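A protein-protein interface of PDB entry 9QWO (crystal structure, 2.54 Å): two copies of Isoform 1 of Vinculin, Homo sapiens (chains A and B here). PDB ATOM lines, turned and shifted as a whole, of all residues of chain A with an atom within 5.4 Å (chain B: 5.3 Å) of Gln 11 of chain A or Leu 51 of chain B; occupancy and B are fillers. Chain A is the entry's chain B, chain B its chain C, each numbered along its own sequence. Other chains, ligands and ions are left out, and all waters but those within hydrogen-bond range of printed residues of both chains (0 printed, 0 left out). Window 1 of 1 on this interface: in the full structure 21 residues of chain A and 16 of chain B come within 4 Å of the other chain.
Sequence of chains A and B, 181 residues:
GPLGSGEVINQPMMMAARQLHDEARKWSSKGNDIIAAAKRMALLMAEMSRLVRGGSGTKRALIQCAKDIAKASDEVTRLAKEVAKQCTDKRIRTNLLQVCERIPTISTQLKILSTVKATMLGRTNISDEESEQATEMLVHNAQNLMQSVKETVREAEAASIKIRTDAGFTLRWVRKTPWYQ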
ATOM      1  N   GLU A   7      18.523  -9.573 -20.268  1.00  0.00           N
ATOM      2  CA  GLU A   7      17.130  -9.953 -20.442  1.00  0.00           C
ATOM      3  C   GLU A   7      16.381  -9.754 -19.128  1.00  0.00           C
ATOM      4  O   GLU A   7      16.990  -9.594 -18.072  1.00  0.00           O
ATOM      5  CB  GLU A   7      16.893 -11.419 -20.818  1.00  0.00           C
ATOM      6  CG  GLU A   7      18.001 -12.041 -21.662  1.00  0.00           C
ATOM      7  CD  GLU A   7      19.008 -12.778 -20.803  1.00  0.00           C
ATOM      8  OE1 GLU A   7      18.765 -13.950 -20.447  1.00  0.00           O
ATOM      9  OE2 GLU A   7      20.027 -12.149 -20.460  1.00  0.00           O
ATOM     10  N   ILE A   9      14.238 -12.064 -17.320  1.00  0.00           N
ATOM     11  CA  ILE A   9      13.850 -13.466 -17.258  1.00  0.00           C
ATOM     12  C   ILE A   9      14.046 -13.995 -15.839  1.00  0.00           C
ATOM     13  O   ILE A   9      14.791 -13.436 -15.038  1.00  0.00           O
ATOM     14  CB  ILE A   9      14.642 -14.316 -18.272  1.00  0.00           C
ATOM     15  CG1 ILE A   9      16.142 -14.359 -17.938  1.00  0.00           C
ATOM     16  CG2 ILE A   9      14.390 -13.830 -19.701  1.00  0.00           C
ATOM     17  CD1 ILE A   9      16.916 -15.455 -18.653  1.00  0.00           C
ATOM     18  N   ASN A  10      13.344 -15.089 -15.540  1.00  0.00           N
ATOM     19  CA  ASN A  10      13.666 -15.913 -14.396  1.00  0.00           C
ATOM     20  C   ASN A  10      14.816 -16.814 -14.821  1.00  0.00           C
ATOM     21  O   ASN A  10      14.650 -17.612 -15.744  1.00  0.00           O
ATOM     22  CB  ASN A  10      12.446 -16.694 -13.924  1.00  0.00           C
ATOM     23  CG  ASN A  10      12.712 -17.406 -12.619  1.00  0.00           C
ATOM     24  OD1 ASN A  10      12.761 -16.768 -11.563  1.00  0.00           O
ATOM     25  ND2 ASN A  10      12.898 -18.715 -12.666  1.00  0.00           N
ATOM     26  N   GLN A  11      15.971 -16.664 -14.155  1.00  0.00           N
ATOM     27  CA  GLN A  11      17.195 -17.308 -14.594  1.00  0.00           C
ATOM     28  C   GLN A  11      17.103 -18.816 -14.363  1.00  0.00           C
ATOM     29  O   GLN A  11      17.426 -19.592 -15.281  1.00  0.00           O
ATOM     30  CB  GLN A  11      18.432 -16.678 -13.949  1.00  0.00           C
ATOM     31  CG  GLN A  11      19.752 -17.214 -14.498  1.00  0.00           C
ATOM     32  CD  GLN A  11      19.938 -16.901 -15.969  1.00  0.00           C
ATOM     33  OE1 GLN A  11      20.204 -15.756 -16.340  1.00  0.00           O
ATOM     34  NE2 GLN A  11      19.806 -17.907 -16.824  1.00  0.00           N
ATOM     35  N   PRO A  12      16.703 -19.297 -13.154  1.00  0.00           N
ATOM     36  CA  PRO A  12      16.641 -20.737 -12.884  1.00  0.00           C
ATOM     37  C   PRO A  12      15.881 -21.524 -13.954  1.00  0.00           C
ATOM     38  O   PRO A  12      16.320 -22.593 -14.375  1.00  0.00           O
ATOM     39  CB  PRO A  12      15.969 -20.785 -11.504  1.00  0.00           C
ATOM     40  CG  PRO A  12      16.428 -19.509 -10.845  1.00  0.00           C
ATOM     41  CD  PRO A  12      16.363 -18.493 -11.968  1.00  0.00           C
ATOM     42  N   MET A  13      14.762 -20.960 -14.419  1.00  0.00           N
ATOM     43  CA  MET A  13      13.905 -21.591 -15.415  1.00  0.00           C
ATOM     44  C   MET A  13      14.587 -21.664 -16.784  1.00  0.00           C
ATOM     45  O   MET A  13      14.415 -22.659 -17.516  1.00  0.00           O
ATOM     46  CB  MET A  13      12.586 -20.832 -15.582  1.00  0.00           C
ATOM     47  CG  MET A  13      11.546 -21.164 -14.519  1.00  0.00           C
ATOM     48  SD  MET A  13      10.055 -20.154 -14.626  1.00  0.00           S
ATOM     49  CE  MET A  13       9.294 -20.855 -16.095  1.00  0.00           C
ATOM     50  N   MET A  14      15.337 -20.606 -17.133  1.00  0.00           N
ATOM     51  CA  MET A  14      16.123 -20.576 -18.360  1.00  0.00           C
ATOM     52  C   MET A  14      17.228 -21.629 -18.288  1.00  0.00           C
ATOM     53  O   MET A  14      17.459 -22.347 -19.262  1.00  0.00           O
ATOM     54  CB  MET A  14      16.708 -19.178 -18.609  1.00  0.00           C
ATOM     55  CG  MET A  14      17.660 -19.076 -19.796  1.00  0.00           C
ATOM     56  SD  MET A  14      16.956 -19.475 -21.409  1.00  0.00           S
ATOM     57  CE  MET A  14      15.978 -17.992 -21.699  1.00  0.00           C
ATOM     58  N   MET A  15      17.893 -21.725 -17.126  1.00  0.00           N
ATOM     59  CA  MET A  15      18.987 -22.667 -16.934  1.00  0.00           C
ATOM     60  C   MET A  15      18.474 -24.095 -17.108  1.00  0.00           C
ATOM     61  O   MET A  15      19.166 -24.937 -17.684  1.00  0.00           O
ATOM     62  CB  MET A  15      19.607 -22.556 -15.537  1.00  0.00           C
ATOM     63  CG  MET A  15      20.671 -21.485 -15.389  1.00  0.00           C
ATOM     64  SD  MET A  15      21.684 -21.770 -13.920  1.00  0.00           S
ATOM     65  CE  MET A  15      22.561 -23.280 -14.351  1.00  0.00           C
ATOM     66  N   ALA A  16      17.272 -24.360 -16.574  1.00  0.00           N
ATOM     67  CA  ALA A  16      16.666 -25.674 -16.697  1.00  0.00           C
ATOM     68  C   ALA A  16      16.424 -25.983 -18.169  1.00  0.00           C
ATOM     69  O   ALA A  16      16.699 -27.092 -18.626  1.00  0.00           O
ATOM     70  CB  ALA A  16      15.390 -25.744 -15.877  1.00  0.00           C
ATOM     71  N   ALA B  46      27.805 -14.930 -16.397  1.00  0.00           N
ATOM     72  CA  ALA B  46      26.738 -13.956 -16.544  1.00  0.00           C
ATOM     73  C   ALA B  46      25.465 -14.445 -15.843  1.00  0.00           C
ATOM     74  O   ALA B  46      24.814 -13.671 -15.150  1.00  0.00           O
ATOM     75  CB  ALA B  46      26.520 -13.667 -18.012  1.00  0.00           C
ATOM     76  N   GLU B  47      25.135 -15.733 -16.010  1.00  0.00           N
ATOM     77  CA  GLU B  47      24.017 -16.362 -15.320  1.00  0.00           C
ATOM     78  C   GLU B  47      24.183 -16.276 -13.798  1.00  0.00           C
ATOM     79  O   GLU B  47      23.239 -15.968 -13.079  1.00  0.00           O
ATOM     80  CB  GLU B  47      23.905 -17.846 -15.679  1.00  0.00           C
ATOM     81  CG  GLU B  47      23.381 -18.139 -17.083  1.00  0.00           C
ATOM     82  CD  GLU B  47      23.393 -19.623 -17.436  1.00  0.00           C
ATOM     83  OE1 GLU B  47      24.180 -20.382 -16.808  1.00  0.00           O
ATOM     84  OE2 GLU B  47      22.615 -20.038 -18.325  1.00  0.00           O
ATOM     85  N   MET B  48      25.395 -16.547 -13.317  1.00  0.00           N
ATOM     86  CA  MET B  48      25.682 -16.588 -11.894  1.00  0.00           C
ATOM     87  C   MET B  48      25.556 -15.192 -11.283  1.00  0.00           C
ATOM     88  O   MET B  48      25.282 -15.058 -10.092  1.00  0.00           O
ATOM     89  CB  MET B  48      27.096 -17.132 -11.660  1.00  0.00           C
ATOM     90  CG  MET B  48      27.284 -17.836 -10.339  1.00  0.00           C
ATOM     91  SD  MET B  48      28.983 -18.408 -10.123  1.00  0.00           S
ATOM     92  CE  MET B  48      28.580 -19.898  -9.201  1.00  0.00           C
ATOM     93  N   SER B  49      25.783 -14.159 -12.099  1.00  0.00           N
ATOM     94  CA  SER B  49      25.704 -12.776 -11.658  1.00  0.00           C
ATOM     95  C   SER B  49      24.265 -12.408 -11.305  1.00  0.00           C
ATOM     96  O   SER B  49      24.038 -11.456 -10.560  1.00  0.00           O
ATOM     97  CB  SER B  49      26.252 -11.833 -12.717  1.00  0.00           C
ATOM     98  OG  SER B  49      25.378 -11.740 -13.839  1.00  0.00           O
ATOM     99  N   ARG B  50      23.309 -13.148 -11.881  1.00  0.00           N
ATOM    100  CA  ARG B  50      21.894 -12.943 -11.631  1.00  0.00           C
ATOM    101  C   ARG B  50      21.414 -13.807 -10.465  1.00  0.00           C
ATOM    102  O   ARG B  50      20.511 -13.408  -9.729  1.00  0.00           O
ATOM    103  CB  ARG B  50      21.091 -13.300 -12.887  1.00  0.00           C
ATOM    104  CG  ARG B  50      21.510 -12.618 -14.184  1.00  0.00           C
ATOM    105  CD  ARG B  50      20.351 -12.608 -15.186  1.00  0.00           C
ATOM    106  NE  ARG B  50      20.708 -12.149 -16.535  1.00  0.00           N
ATOM    107  CZ  ARG B  50      21.464 -12.807 -17.415  1.00  0.00           C
ATOM    108  NH1 ARG B  50      21.815 -12.228 -18.554  1.00  0.00           N
ATOM    109  NH2 ARG B  50      21.899 -14.027 -17.152  1.00  0.00           N
ATOM    110  N   LEU B  51      22.007 -15.000 -10.321  1.00  0.00           N
ATOM    111  CA  LEU B  51      21.549 -15.992  -9.361  1.00  0.00           C
ATOM    112  C   LEU B  51      21.945 -15.604  -7.936  1.00  0.00           C
ATOM    113  O   LEU B  51      21.259 -15.975  -6.984  1.00  0.00           O
ATOM    114  CB  LEU B  51      22.127 -17.353  -9.743  1.00  0.00           C
ATOM    115  CG  LEU B  51      21.618 -17.959 -11.054  1.00  0.00           C
ATOM    116  CD1 LEU B  51      22.394 -19.213 -11.377  1.00  0.00           C
ATOM    117  CD2 LEU B  51      20.135 -18.265 -11.006  1.00  0.00           C
ATOM    118  N   VAL B  52      23.055 -14.865  -7.799  1.00  0.00           N
ATOM    119  CA  VAL B  52      23.577 -14.469  -6.497  1.00  0.00           C
ATOM    120  C   VAL B  52      22.664 -13.432  -5.840  1.00  0.00           C
ATOM    121  O   VAL B  52      22.817 -13.143  -4.657  1.00  0.00           O
ATOM    122  CB  VAL B  52      25.025 -13.959  -6.664  1.00  0.00           C
ATOM    123  CG1 VAL B  52      25.453 -12.977  -5.579  1.00  0.00           C
ATOM    124  CG2 VAL B  52      26.011 -15.117  -6.747  1.00  0.00           C
ATOM    125  N   ARG B  53      21.705 -12.888  -6.600  1.00  0.00           N
ATOM    126  CA  ARG B  53      20.796 -11.863  -6.105  1.00  0.00           C
ATOM    127  C   ARG B  53      19.592 -12.468  -5.379  1.00  0.00           C
ATOM    128  O   ARG B  53      18.664 -11.736  -5.042  1.00  0.00           O
ATOM    129  CB  ARG B  53      20.250 -11.011  -7.258  1.00  0.00           C
ATOM    130  CG  ARG B  53      21.297 -10.426  -8.196  1.00  0.00           C
ATOM    131  CD  ARG B  53      22.472  -9.776  -7.470  1.00  0.00           C
ATOM    132  NE  ARG B  53      22.063  -8.800  -6.451  1.00  0.00           N
ATOM    133  CZ  ARG B  53      22.882  -8.252  -5.555  1.00  0.00           C
ATOM    134  NH1 ARG B  53      22.383  -7.529  -4.563  1.00  0.00           N
ATOM    135  NH2 ARG B  53      24.191  -8.467  -5.625  1.00  0.00           N
ATOM    136  N   GLY B  54      19.601 -13.788  -5.142  1.00  0.00           N
ATOM    137  CA  GLY B  54      18.455 -14.475  -4.571  1.00  0.00           C
ATOM    138  C   GLY B  54      17.303 -14.534  -5.573  1.00  0.00           C
ATOM    139  O   GLY B  54      17.446 -14.083  -6.709  1.00  0.00           O
ATOM    140  N   THR B  58      16.716 -20.272  -6.927  1.00  0.00           N
ATOM    141  CA  THR B  58      18.099 -19.827  -6.938  1.00  0.00           C
ATOM    142  C   THR B  58      19.033 -20.880  -6.349  1.00  0.00           C
ATOM    143  O   THR B  58      20.087 -21.140  -6.934  1.00  0.00           O
ATOM    144  CB  THR B  58      18.244 -18.503  -6.165  1.00  0.00           C
ATOM    145  OG1 THR B  58      17.810 -18.687  -4.813  1.00  0.00           O
ATOM    146  CG2 THR B  58      17.276 -17.461  -6.704  1.00  0.00           C
ATOM    147  N   ALA B  61      19.811 -23.726  -8.759  1.00  0.00           N
ATOM    148  CA  ALA B  61      20.400 -23.261 -10.006  1.00  0.00           C
ATOM    149  C   ALA B  61      21.839 -22.784  -9.797  1.00  0.00           C
ATOM    150  O   ALA B  61      22.674 -22.953 -10.678  1.00  0.00           O
ATOM    151  CB  ALA B  61      19.551 -22.163 -10.592  1.00  0.00           C
ATOM    152  N   LEU B  62      22.111 -22.192  -8.627  1.00  0.00           N
ATOM    153  CA  LEU B  62      23.420 -21.645  -8.290  1.00  0.00           C
ATOM    154  C   LEU B  62      24.434 -22.756  -8.011  1.00  0.00           C
ATOM    155  O   LEU B  62      25.629 -22.567  -8.243  1.00  0.00           O
ATOM    156  CB  LEU B  62      23.258 -20.719  -7.085  1.00  0.00           C
ATOM    157  CG  LEU B  62      24.521 -20.028  -6.569  1.00  0.00           C
ATOM    158  CD1 LEU B  62      25.278 -19.283  -7.648  1.00  0.00           C
ATOM    159  CD2 LEU B  62      24.139 -19.079  -5.451  1.00  0.00           C
ATOM    160  N   CYS B  65      24.958 -24.415 -11.447  1.00  0.00           N
ATOM    161  CA  CYS B  65      25.712 -23.491 -12.273  1.00  0.00           C
ATOM    162  C   CYS B  65      27.209 -23.650 -12.024  1.00  0.00           C
ATOM    163  O   CYS B  65      27.988 -23.738 -12.977  1.00  0.00           O
ATOM    164  CB  CYS B  65      25.302 -22.047 -12.021  1.00  0.00           C
ATOM    165  SG  CYS B  65      26.243 -20.882 -13.036  1.00  0.00           S
ATOM    166  N   LEU B 121      20.801 -18.258   1.021  1.00  0.00           N
ATOM    167  CA  LEU B 121      19.651 -17.588   0.438  1.00  0.00           C
ATOM    168  C   LEU B 121      18.380 -18.107   1.105  1.00  0.00           C
ATOM    169  O   LEU B 121      18.262 -19.302   1.380  1.00  0.00           O
ATOM    170  CB  LEU B 121      19.629 -17.811  -1.072  1.00  0.00           C
ATOM    171  CG  LEU B 121      20.792 -17.193  -1.857  1.00  0.00           C
ATOM    172  CD1 LEU B 121      20.841 -17.738  -3.270  1.00  0.00           C
ATOM    173  CD2 LEU B 121      20.717 -15.675  -1.886  1.00  0.00           C
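NE2 of Gln 11 of chain A touches CG of Glu 47 of chain B, at 3.6 Å. Leu 51 of chain B touches Gln 11 of chain A (CD2 to CG, 3.7 Å). Leu 51 of chain B touches Pro 12 of chain A. CB of Pro 12 of chain A touches CB of Ala 61 of chain B (3.9 Å). Met 15 of chain A touches Glu 47 of chain B (CG to OE2, 3.8 Å). Met 15 of chain A touches Leu 51 of chain B (SD to CD1, 3.7 Å). Cys 65 of chain B touches Met 15 of chain A (CA to CE, 3.8 Å).
The guanidinium group (NH1) of Arg 50 of chain B is in salt-bridge range of the side-chain carboxylate (OE2) of Glu 7 of chain A. The guanidinium group (NH2) of Arg 50 of chain B is in hydrogen-bond range of the side-chain amide oxygen (OE1) of Gln 11 of chain A, 2.6 Å away. The side-chain sulfur (SD) of Met 15 of chain A lies close to the backbone carbonyl oxygen (O) of Ala 61 of chain B (3.6 Å).
No position is printed for both chains. Of the 10 pairs that touch across the chains among the printed residues, none has its exchanged pair printed and touching as well.
Gln 11 of chain A touches three residues of chain B. Leu 51 of chain B touches three residues of chain A. Of the printed residues of chain B, Met 15 of chain A touches Glu 47 (3.8 Å), Leu 51 (3.7 Å), Ala 61 (3.6 Å) and Cys 65 (3.8 Å). Of the printed residues of chain A, Cys 65 of chain B touches Met 15. Gly 54 of chain B touches none of the printed residues of chain A. The nearest residue of chain B that does not touch Gln 11 of chain A is Ala 46 of chain B (5.2 Å). The nearest printed residue of chain A that does not touch Ala 61 of chain B is Gln 11 of chain A (5.6 Å).
Printed residues of chain B that touch a printed residue of chain A: Glu 47, Arg 50, Leu 51, Ala 61 and Cys 65. Hydrophobic or aromatic side chains of chain B that line the printed part of chain A: Leu 51 and Ala 61. Among the printed residues, 10 pairs touch across the chains. Among the printed residues, Asp or Glu carboxylates within 4 Å of a Lys or Arg side-chain nitrogen of the other chain: Glu 7 of chain A with Arg 50 of chain B.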
